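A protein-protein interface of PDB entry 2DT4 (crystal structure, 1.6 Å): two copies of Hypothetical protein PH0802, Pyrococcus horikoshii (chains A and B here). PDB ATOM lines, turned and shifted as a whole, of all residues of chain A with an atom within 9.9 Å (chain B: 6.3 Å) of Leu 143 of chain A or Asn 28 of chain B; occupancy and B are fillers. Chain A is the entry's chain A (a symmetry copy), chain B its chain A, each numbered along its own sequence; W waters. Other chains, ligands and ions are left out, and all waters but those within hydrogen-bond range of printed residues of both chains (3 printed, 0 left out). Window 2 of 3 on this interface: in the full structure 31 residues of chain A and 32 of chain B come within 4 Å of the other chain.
The side-chain hydroxyl (OH) of Tyr 25 of chain B is in hydrogen-bond range of the backbone carbonyl oxygen (O) of Leu 141 of chain A (2.7 Å).
No position is printed for both chains.
Among the printed residues, merely in contact across the chains: Leu 141 of chain A with Pro 17 of chain B (3.3 Å), Leu 143 of chain A with Tyr 25 of chain B (3.5 Å), Glu 140 of chain A with Pro 17 of chain B (3.6 Å), Leu 143 of chain A with Phe 29 of chain B (3.6 Å), Leu 141 of chain A with Phe 29 of chain B (3.8 Å) and Leu 143 of chain A with Asn 28 of chain B (3.8 Å).
Water W2 bridges OE2 of Glu 20 of chain B (2.7 Å) and NZ of Lys 142 of chain A (2.9 Å). Water W1 lies within hydrogen-bond range of O of Thr 3 of chain A and OE1 of Glu 33 of chain B. Water W3 bridges OE2 of Glu 20 of chain B (2.9 Å) and N of Leu 143 of chain A (2.9 Å).
Of the printed residues of chain B, Glu 140 of chain A touches Pro 17. Leu 143 of chain A touches three residues of chain B. Printed residues of chain A within 4 Å of Pro 17 of chain B: Glu 140 and Leu 141. Ile 26 of chain B touches none of the printed residues of chain A. Asn 28 of chain B touches just one residue of chain A: Leu 143. No residue of chain A comes within 4 Å of Lys 31 of chain B.
Of the 14 printed residues of chain B, 4 touch a printed residue of chain A. Hydrophobic or aromatic side chains of chain B within 4 Å of the printed part of chain A: Pro 17, Tyr 25 and Phe 29. Of the 8 printed residues of chain A, 3 touch a printed residue of chain B. Printed residues of chain A that touch a printed residue of chain B: Glu 140, Leu 141 and Leu 143.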
ATOM      1  N   MET A   1      21.472   7.729 -22.274  1.00  0.00           N
ATOM      2  CA  MET A   1      21.297   8.283 -20.906  1.00  0.00           C
ATOM      3  C   MET A   1      21.320   9.806 -20.968  1.00  0.00           C
ATOM      4  O   MET A   1      22.216  10.364 -21.610  1.00  0.00           O
ATOM      5  CB  MET A   1      22.218   7.662 -19.885  1.00  0.00           C
ATOM      6  CG  MET A   1      23.271   8.454 -19.183  1.00  0.00           C
ATOM      7  SD  MET A   1      24.155   7.745 -17.845  1.00  0.00           S
ATOM      8  CE  MET A   1      25.576   8.865 -17.781  1.00  0.00           C
ATOM      9  N   VAL A   2      20.493  10.433 -20.174  1.00  0.00           N
ATOM     10  CA  VAL A   2      20.482  11.894 -20.115  1.00  0.00           C
ATOM     11  C   VAL A   2      21.691  12.379 -19.310  1.00  0.00           C
ATOM     12  O   VAL A   2      21.914  11.933 -18.195  1.00  0.00           O
ATOM     13  CB  VAL A   2      19.162  12.376 -19.489  1.00  0.00           C
ATOM     14  CG1 VAL A   2      19.138  13.901 -19.360  1.00  0.00           C
ATOM     15  CG2 VAL A   2      17.996  11.898 -20.332  1.00  0.00           C
ATOM     16  N   THR A   3      22.484  13.273 -19.877  1.00  0.00           N
ATOM     17  CA  THR A   3      23.514  13.957 -19.099  1.00  0.00           C
ATOM     18  C   THR A   3      23.246  15.432 -18.897  1.00  0.00           C
ATOM     19  O   THR A   3      23.810  16.019 -18.011  1.00  0.00           O
ATOM     20  CB  THR A   3      24.907  13.817 -19.723  1.00  0.00           C
ATOM     21  OG1 THR A   3      25.017  14.608 -20.922  1.00  0.00           O
ATOM     22  CG2 THR A   3      25.156  12.379 -20.185  1.00  0.00           C
ATOM     23  N   GLY A   4      22.452  16.040 -19.766  1.00  0.00           N
ATOM     24  CA  GLY A   4      22.189  17.447 -19.680  1.00  0.00           C
ATOM     25  C   GLY A   4      23.330  18.333 -20.123  1.00  0.00           C
ATOM     26  O   GLY A   4      23.198  19.547 -20.010  1.00  0.00           O
ATOM     27  N   GLU A 140      13.787  13.763 -17.839  1.00  0.00           N
ATOM     28  CA  GLU A 140      14.427  14.402 -16.701  1.00  0.00           C
ATOM     29  C   GLU A 140      15.850  13.925 -16.495  1.00  0.00           C
ATOM     30  O   GLU A 140      16.242  12.816 -16.934  1.00  0.00           O
ATOM     31  CB  GLU A 140      13.618  14.126 -15.447  1.00  0.00           C
ATOM     32  CG  GLU A 140      13.721  12.688 -14.933  1.00  0.00           C
ATOM     33  CD  GLU A 140      12.691  12.383 -13.860  1.00  0.00           C
ATOM     34  OE1 GLU A 140      12.875  11.389 -13.136  1.00  0.00           O
ATOM     35  OE2 GLU A 140      11.706  13.127 -13.738  1.00  0.00           O
ATOM     36  N   LEU A 141      16.599  14.755 -15.761  1.00  0.00           N
ATOM     37  CA  LEU A 141      17.973  14.427 -15.388  1.00  0.00           C
ATOM     38  C   LEU A 141      17.910  13.951 -13.933  1.00  0.00           C
ATOM     39  O   LEU A 141      17.773  14.733 -12.999  1.00  0.00           O
ATOM     40  CB  LEU A 141      18.939  15.598 -15.571  1.00  0.00           C
ATOM     41  CG  LEU A 141      20.384  15.368 -15.117  1.00  0.00           C
ATOM     42  CD1 LEU A 141      21.009  14.241 -15.917  1.00  0.00           C
ATOM     43  CD2 LEU A 141      21.212  16.607 -15.272  1.00  0.00           C
ATOM     44  N   LYS A 142      17.967  12.631 -13.748  1.00  0.00           N
ATOM     45  CA  LYS A 142      17.842  12.056 -12.414  1.00  0.00           C
ATOM     46  C   LYS A 142      19.255  11.876 -11.887  1.00  0.00           C
ATOM     47  O   LYS A 142      20.060  11.194 -12.521  1.00  0.00           O
ATOM     48  CB  LYS A 142      17.127  10.702 -12.511  1.00  0.00           C
ATOM     49  CG  LYS A 142      16.910  10.028 -11.148  1.00  0.00           C
ATOM     50  CD  LYS A 142      15.631  10.499 -10.508  1.00  0.00           C
ATOM     51  CE  LYS A 142      15.211   9.639  -9.328  1.00  0.00           C
ATOM     52  NZ  LYS A 142      14.169  10.420  -8.586  1.00  0.00           N
ATOM     53  N   LEU A 143      19.573  12.485 -10.736  1.00  0.00           N
ATOM     54  CA  LEU A 143      20.902  12.353 -10.134  1.00  0.00           C
ATOM     55  C   LEU A 143      21.113  10.967  -9.515  1.00  0.00           C
ATOM     56  O   LEU A 143      22.276  10.594  -9.400  1.00  0.00           O
ATOM     57  CB  LEU A 143      21.125  13.415  -9.064  1.00  0.00           C
ATOM     58  CG  LEU A 143      21.061  14.862  -9.546  1.00  0.00           C
ATOM     59  CD1 LEU A 143      21.289  15.837  -8.385  1.00  0.00           C
ATOM     60  CD2 LEU A 143      22.060  15.141 -10.676  1.00  0.00           C
ATOM     61  OXT LEU A 143      20.119  10.319  -9.158  1.00  0.00           O
ATOM     62  N   PRO B  17      13.759  16.624 -11.829  1.00  0.00           N
ATOM     63  CA  PRO B  17      12.625  15.762 -11.491  1.00  0.00           C
ATOM     64  C   PRO B  17      11.591  16.387 -10.557  1.00  0.00           C
ATOM     65  O   PRO B  17      11.931  17.109  -9.620  1.00  0.00           O
ATOM     66  CB  PRO B  17      13.301  14.560 -10.830  1.00  0.00           C
ATOM     67  CG  PRO B  17      14.602  14.495 -11.448  1.00  0.00           C
ATOM     68  CD  PRO B  17      15.033  15.948 -11.586  1.00  0.00           C
ATOM     69  N   GLU B  20      11.758  17.300  -6.375  1.00  0.00           N
ATOM     70  CA  GLU B  20      13.034  17.729  -5.804  1.00  0.00           C
ATOM     71  C   GLU B  20      12.799  19.097  -5.212  1.00  0.00           C
ATOM     72  O   GLU B  20      11.960  19.867  -5.740  1.00  0.00           O
ATOM     73  CB  GLU B  20      14.110  17.849  -6.890  1.00  0.00           C
ATOM     74  CG  GLU B  20      14.633  16.499  -7.339  1.00  0.00           C
ATOM     75  CD  GLU B  20      15.839  15.991  -6.535  1.00  0.00           C
ATOM     76  OE1 GLU B  20      16.357  16.662  -5.621  1.00  0.00           O
ATOM     77  OE2 GLU B  20      16.307  14.878  -6.862  1.00  0.00           O
ATOM     78  N   LEU B  23      16.795  24.206  -4.974  1.00  0.00           N
ATOM     79  CA  LEU B  23      18.134  24.642  -4.550  1.00  0.00           C
ATOM     80  C   LEU B  23      18.994  23.436  -4.203  1.00  0.00           C
ATOM     81  O   LEU B  23      20.164  23.355  -4.606  1.00  0.00           O
ATOM     82  CB  LEU B  23      18.128  25.664  -3.387  1.00  0.00           C
ATOM     83  CG  LEU B  23      17.474  27.010  -3.714  1.00  0.00           C
ATOM     84  CD1 LEU B  23      17.337  27.794  -2.429  1.00  0.00           C
ATOM     85  CD2 LEU B  23      18.277  27.793  -4.741  1.00  0.00           C
ATOM     86  N   THR B  24      18.383  22.480  -3.509  1.00  0.00           N
ATOM     87  CA  THR B  24      19.053  21.253  -3.117  1.00  0.00           C
ATOM     88  C   THR B  24      19.523  20.496  -4.326  1.00  0.00           C
ATOM     89  O   THR B  24      20.674  20.081  -4.383  1.00  0.00           O
ATOM     90  CB  THR B  24      18.114  20.421  -2.245  1.00  0.00           C
ATOM     91  OG1 THR B  24      17.817  21.159  -1.052  1.00  0.00           O
ATOM     92  CG2 THR B  24      18.806  19.142  -1.762  1.00  0.00           C
ATOM     93  N   TYR B  25      18.667  20.344  -5.331  1.00  0.00           N
ATOM     94  CA  TYR B  25      19.045  19.597  -6.520  1.00  0.00           C
ATOM     95  C   TYR B  25      20.210  20.279  -7.234  1.00  0.00           C
ATOM     96  O   TYR B  25      21.155  19.637  -7.634  1.00  0.00           O
ATOM     97  CB  TYR B  25      17.854  19.462  -7.483  1.00  0.00           C
ATOM     98  CG  TYR B  25      18.181  18.804  -8.797  1.00  0.00           C
ATOM     99  CD1 TYR B  25      17.918  17.456  -9.022  1.00  0.00           C
ATOM    100  CD2 TYR B  25      18.776  19.522  -9.820  1.00  0.00           C
ATOM    101  CE1 TYR B  25      18.219  16.866 -10.232  1.00  0.00           C
ATOM    102  CE2 TYR B  25      19.082  18.939 -11.026  1.00  0.00           C
ATOM    103  CZ  TYR B  25      18.801  17.619 -11.221  1.00  0.00           C
ATOM    104  OH  TYR B  25      19.078  17.056 -12.429  1.00  0.00           O
ATOM    105  N   ILE B  26      20.155  21.600  -7.369  1.00  0.00           N
ATOM    106  CA  ILE B  26      21.186  22.281  -8.129  1.00  0.00           C
ATOM    107  C   ILE B  26      22.513  22.106  -7.376  1.00  0.00           C
ATOM    108  O   ILE B  26      23.524  21.839  -8.005  1.00  0.00           O
ATOM    109  CB  ILE B  26      20.847  23.782  -8.412  1.00  0.00           C
ATOM    110  CG1 ILE B  26      19.645  23.886  -9.356  1.00  0.00           C
ATOM    111  CG2 ILE B  26      22.069  24.490  -9.023  1.00  0.00           C
ATOM    112  CD1 ILE B  26      19.038  25.225  -9.383  1.00  0.00           C
ATOM    113  N   LYS B  27      22.499  22.219  -6.044  1.00  0.00           N
ATOM    114  CA  LYS B  27      23.692  21.980  -5.223  1.00  0.00           C
ATOM    115  C   LYS B  27      24.251  20.570  -5.430  1.00  0.00           C
ATOM    116  O   LYS B  27      25.458  20.389  -5.684  1.00  0.00           O
ATOM    117  CB  LYS B  27      23.394  22.215  -3.748  1.00  0.00           C
ATOM    118  CG  LYS B  27      24.576  21.857  -2.844  1.00  0.00           C
ATOM    119  CD  LYS B  27      24.337  22.228  -1.372  1.00  0.00           C
ATOM    120  CE  LYS B  27      25.520  21.807  -0.542  1.00  0.00           C
ATOM    121  NZ  LYS B  27      25.705  22.453   0.810  1.00  0.00           N
ATOM    122  N   ASN B  28      23.372  19.568  -5.354  1.00  0.00           N
ATOM    123  CA  ASN B  28      23.793  18.182  -5.509  1.00  0.00           C
ATOM    124  C   ASN B  28      24.321  17.882  -6.921  1.00  0.00           C
ATOM    125  O   ASN B  28      25.265  17.089  -7.110  1.00  0.00           O
ATOM    126  CB  ASN B  28      22.618  17.259  -5.143  1.00  0.00           C
ATOM    127  CG  ASN B  28      22.402  17.183  -3.619  1.00  0.00           C
ATOM    128  OD1 ASN B  28      23.341  17.449  -2.842  1.00  0.00           O
ATOM    129  ND2 ASN B  28      21.189  16.830  -3.190  1.00  0.00           N
ATOM    130  N   PHE B  29      23.672  18.481  -7.914  1.00  0.00           N
ATOM    131  CA  PHE B  29      24.146  18.417  -9.296  1.00  0.00           C
ATOM    132  C   PHE B  29      25.615  18.942  -9.356  1.00  0.00           C
ATOM    133  O   PHE B  29      26.498  18.282  -9.931  1.00  0.00           O
ATOM    134  CB  PHE B  29      23.204  19.177 -10.226  1.00  0.00           C
ATOM    135  CG  PHE B  29      23.739  19.378 -11.604  1.00  0.00           C
ATOM    136  CD1 PHE B  29      24.476  20.515 -11.880  1.00  0.00           C
ATOM    137  CD2 PHE B  29      23.500  18.476 -12.626  1.00  0.00           C
ATOM    138  CE1 PHE B  29      24.957  20.745 -13.139  1.00  0.00           C
ATOM    139  CE2 PHE B  29      24.024  18.721 -13.890  1.00  0.00           C
ATOM    140  CZ  PHE B  29      24.780  19.852 -14.097  1.00  0.00           C
ATOM    141  N   CYS B  30      25.861  20.130  -8.813  1.00  0.00           N
ATOM    142  CA  CYS B  30      27.181  20.715  -8.869  1.00  0.00           C
ATOM    143  C   CYS B  30      28.171  19.844  -8.092  1.00  0.00           C
ATOM    144  O   CYS B  30      29.280  19.680  -8.531  1.00  0.00           O
ATOM    145  CB  CYS B  30      27.197  22.160  -8.367  1.00  0.00           C
ATOM    146  SG  CYS B  30      26.286  23.285  -9.458  1.00  0.00           S
ATOM    147  N   LYS B  31      27.765  19.263  -6.964  1.00  0.00           N
ATOM    148  CA  LYS B  31      28.686  18.375  -6.241  1.00  0.00           C
ATOM    149  C   LYS B  31      29.106  17.193  -7.078  1.00  0.00           C
ATOM    150  O   LYS B  31      30.305  16.851  -7.132  1.00  0.00           O
ATOM    151  CB  LYS B  31      28.084  17.917  -4.922  1.00  0.00           C
ATOM    152  CG  LYS B  31      27.994  19.016  -3.924  1.00  0.00           C
ATOM    153  CD  LYS B  31      27.470  18.485  -2.594  1.00  0.00           C
ATOM    154  CE  LYS B  31      27.418  19.594  -1.617  1.00  0.00           C
ATOM    155  NZ  LYS B  31      26.927  19.128  -0.265  1.00  0.00           N
ATOM    156  N   LYS B  32      28.137  16.584  -7.744  1.00  0.00           N
ATOM    157  CA  LYS B  32      28.385  15.448  -8.593  1.00  0.00           C
ATOM    158  C   LYS B  32      29.312  15.809  -9.741  1.00  0.00           C
ATOM    159  O   LYS B  32      30.253  15.070 -10.049  1.00  0.00           O
ATOM    160  CB  LYS B  32      27.082  14.882  -9.143  1.00  0.00           C
ATOM    161  CG  LYS B  32      27.298  13.633  -9.982  1.00  0.00           C
ATOM    162  CD  LYS B  32      28.172  12.610  -9.302  1.00  0.00           C
ATOM    163  CE  LYS B  32      28.250  11.326 -10.114  1.00  0.00           C
ATOM    164  NZ  LYS B  32      28.631  11.577 -11.547  1.00  0.00           N
ATOM    165  N   GLU B  33      29.064  16.946 -10.375  1.00  0.00           N
ATOM    166  CA  GLU B  33      29.841  17.350 -11.546  1.00  0.00           C
ATOM    167  C   GLU B  33      31.174  17.997 -11.200  1.00  0.00           C
ATOM    168  O   GLU B  33      31.973  18.291 -12.093  1.00  0.00           O
ATOM    169  CB  GLU B  33      29.028  18.342 -12.383  1.00  0.00           C
ATOM    170  CG  GLU B  33      27.779  17.755 -12.997  1.00  0.00           C
ATOM    171  CD  GLU B  33      28.105  16.738 -14.064  1.00  0.00           C
ATOM    172  OE1 GLU B  33      27.696  15.575 -13.886  1.00  0.00           O
ATOM    173  OE2 GLU B  33      28.818  17.049 -15.041  1.00  0.00           O
ATOM    174  N   VAL B  88      24.268  27.642  -3.729  1.00  0.00           N
ATOM    175  CA  VAL B  88      23.339  28.158  -4.730  1.00  0.00           C
ATOM    176  C   VAL B  88      22.599  29.374  -4.173  1.00  0.00           C
ATOM    177  O   VAL B  88      22.002  29.319  -3.095  1.00  0.00           O
ATOM    178  CB  VAL B  88      22.344  27.079  -5.174  1.00  0.00           C
ATOM    179  CG1 VAL B  88      21.582  27.557  -6.419  1.00  0.00           C
ATOM    180  CG2 VAL B  88      23.066  25.767  -5.453  1.00  0.00           C
HETATM  181  O   HOH W   1      25.234  14.762 -16.087  1.00  0.00           O
HETATM  182  O   HOH W   2      14.595  12.872  -7.167  1.00  0.00           O
HETATM  183  O   HOH W   3      17.370  13.519  -9.149  1.00  0.00           O
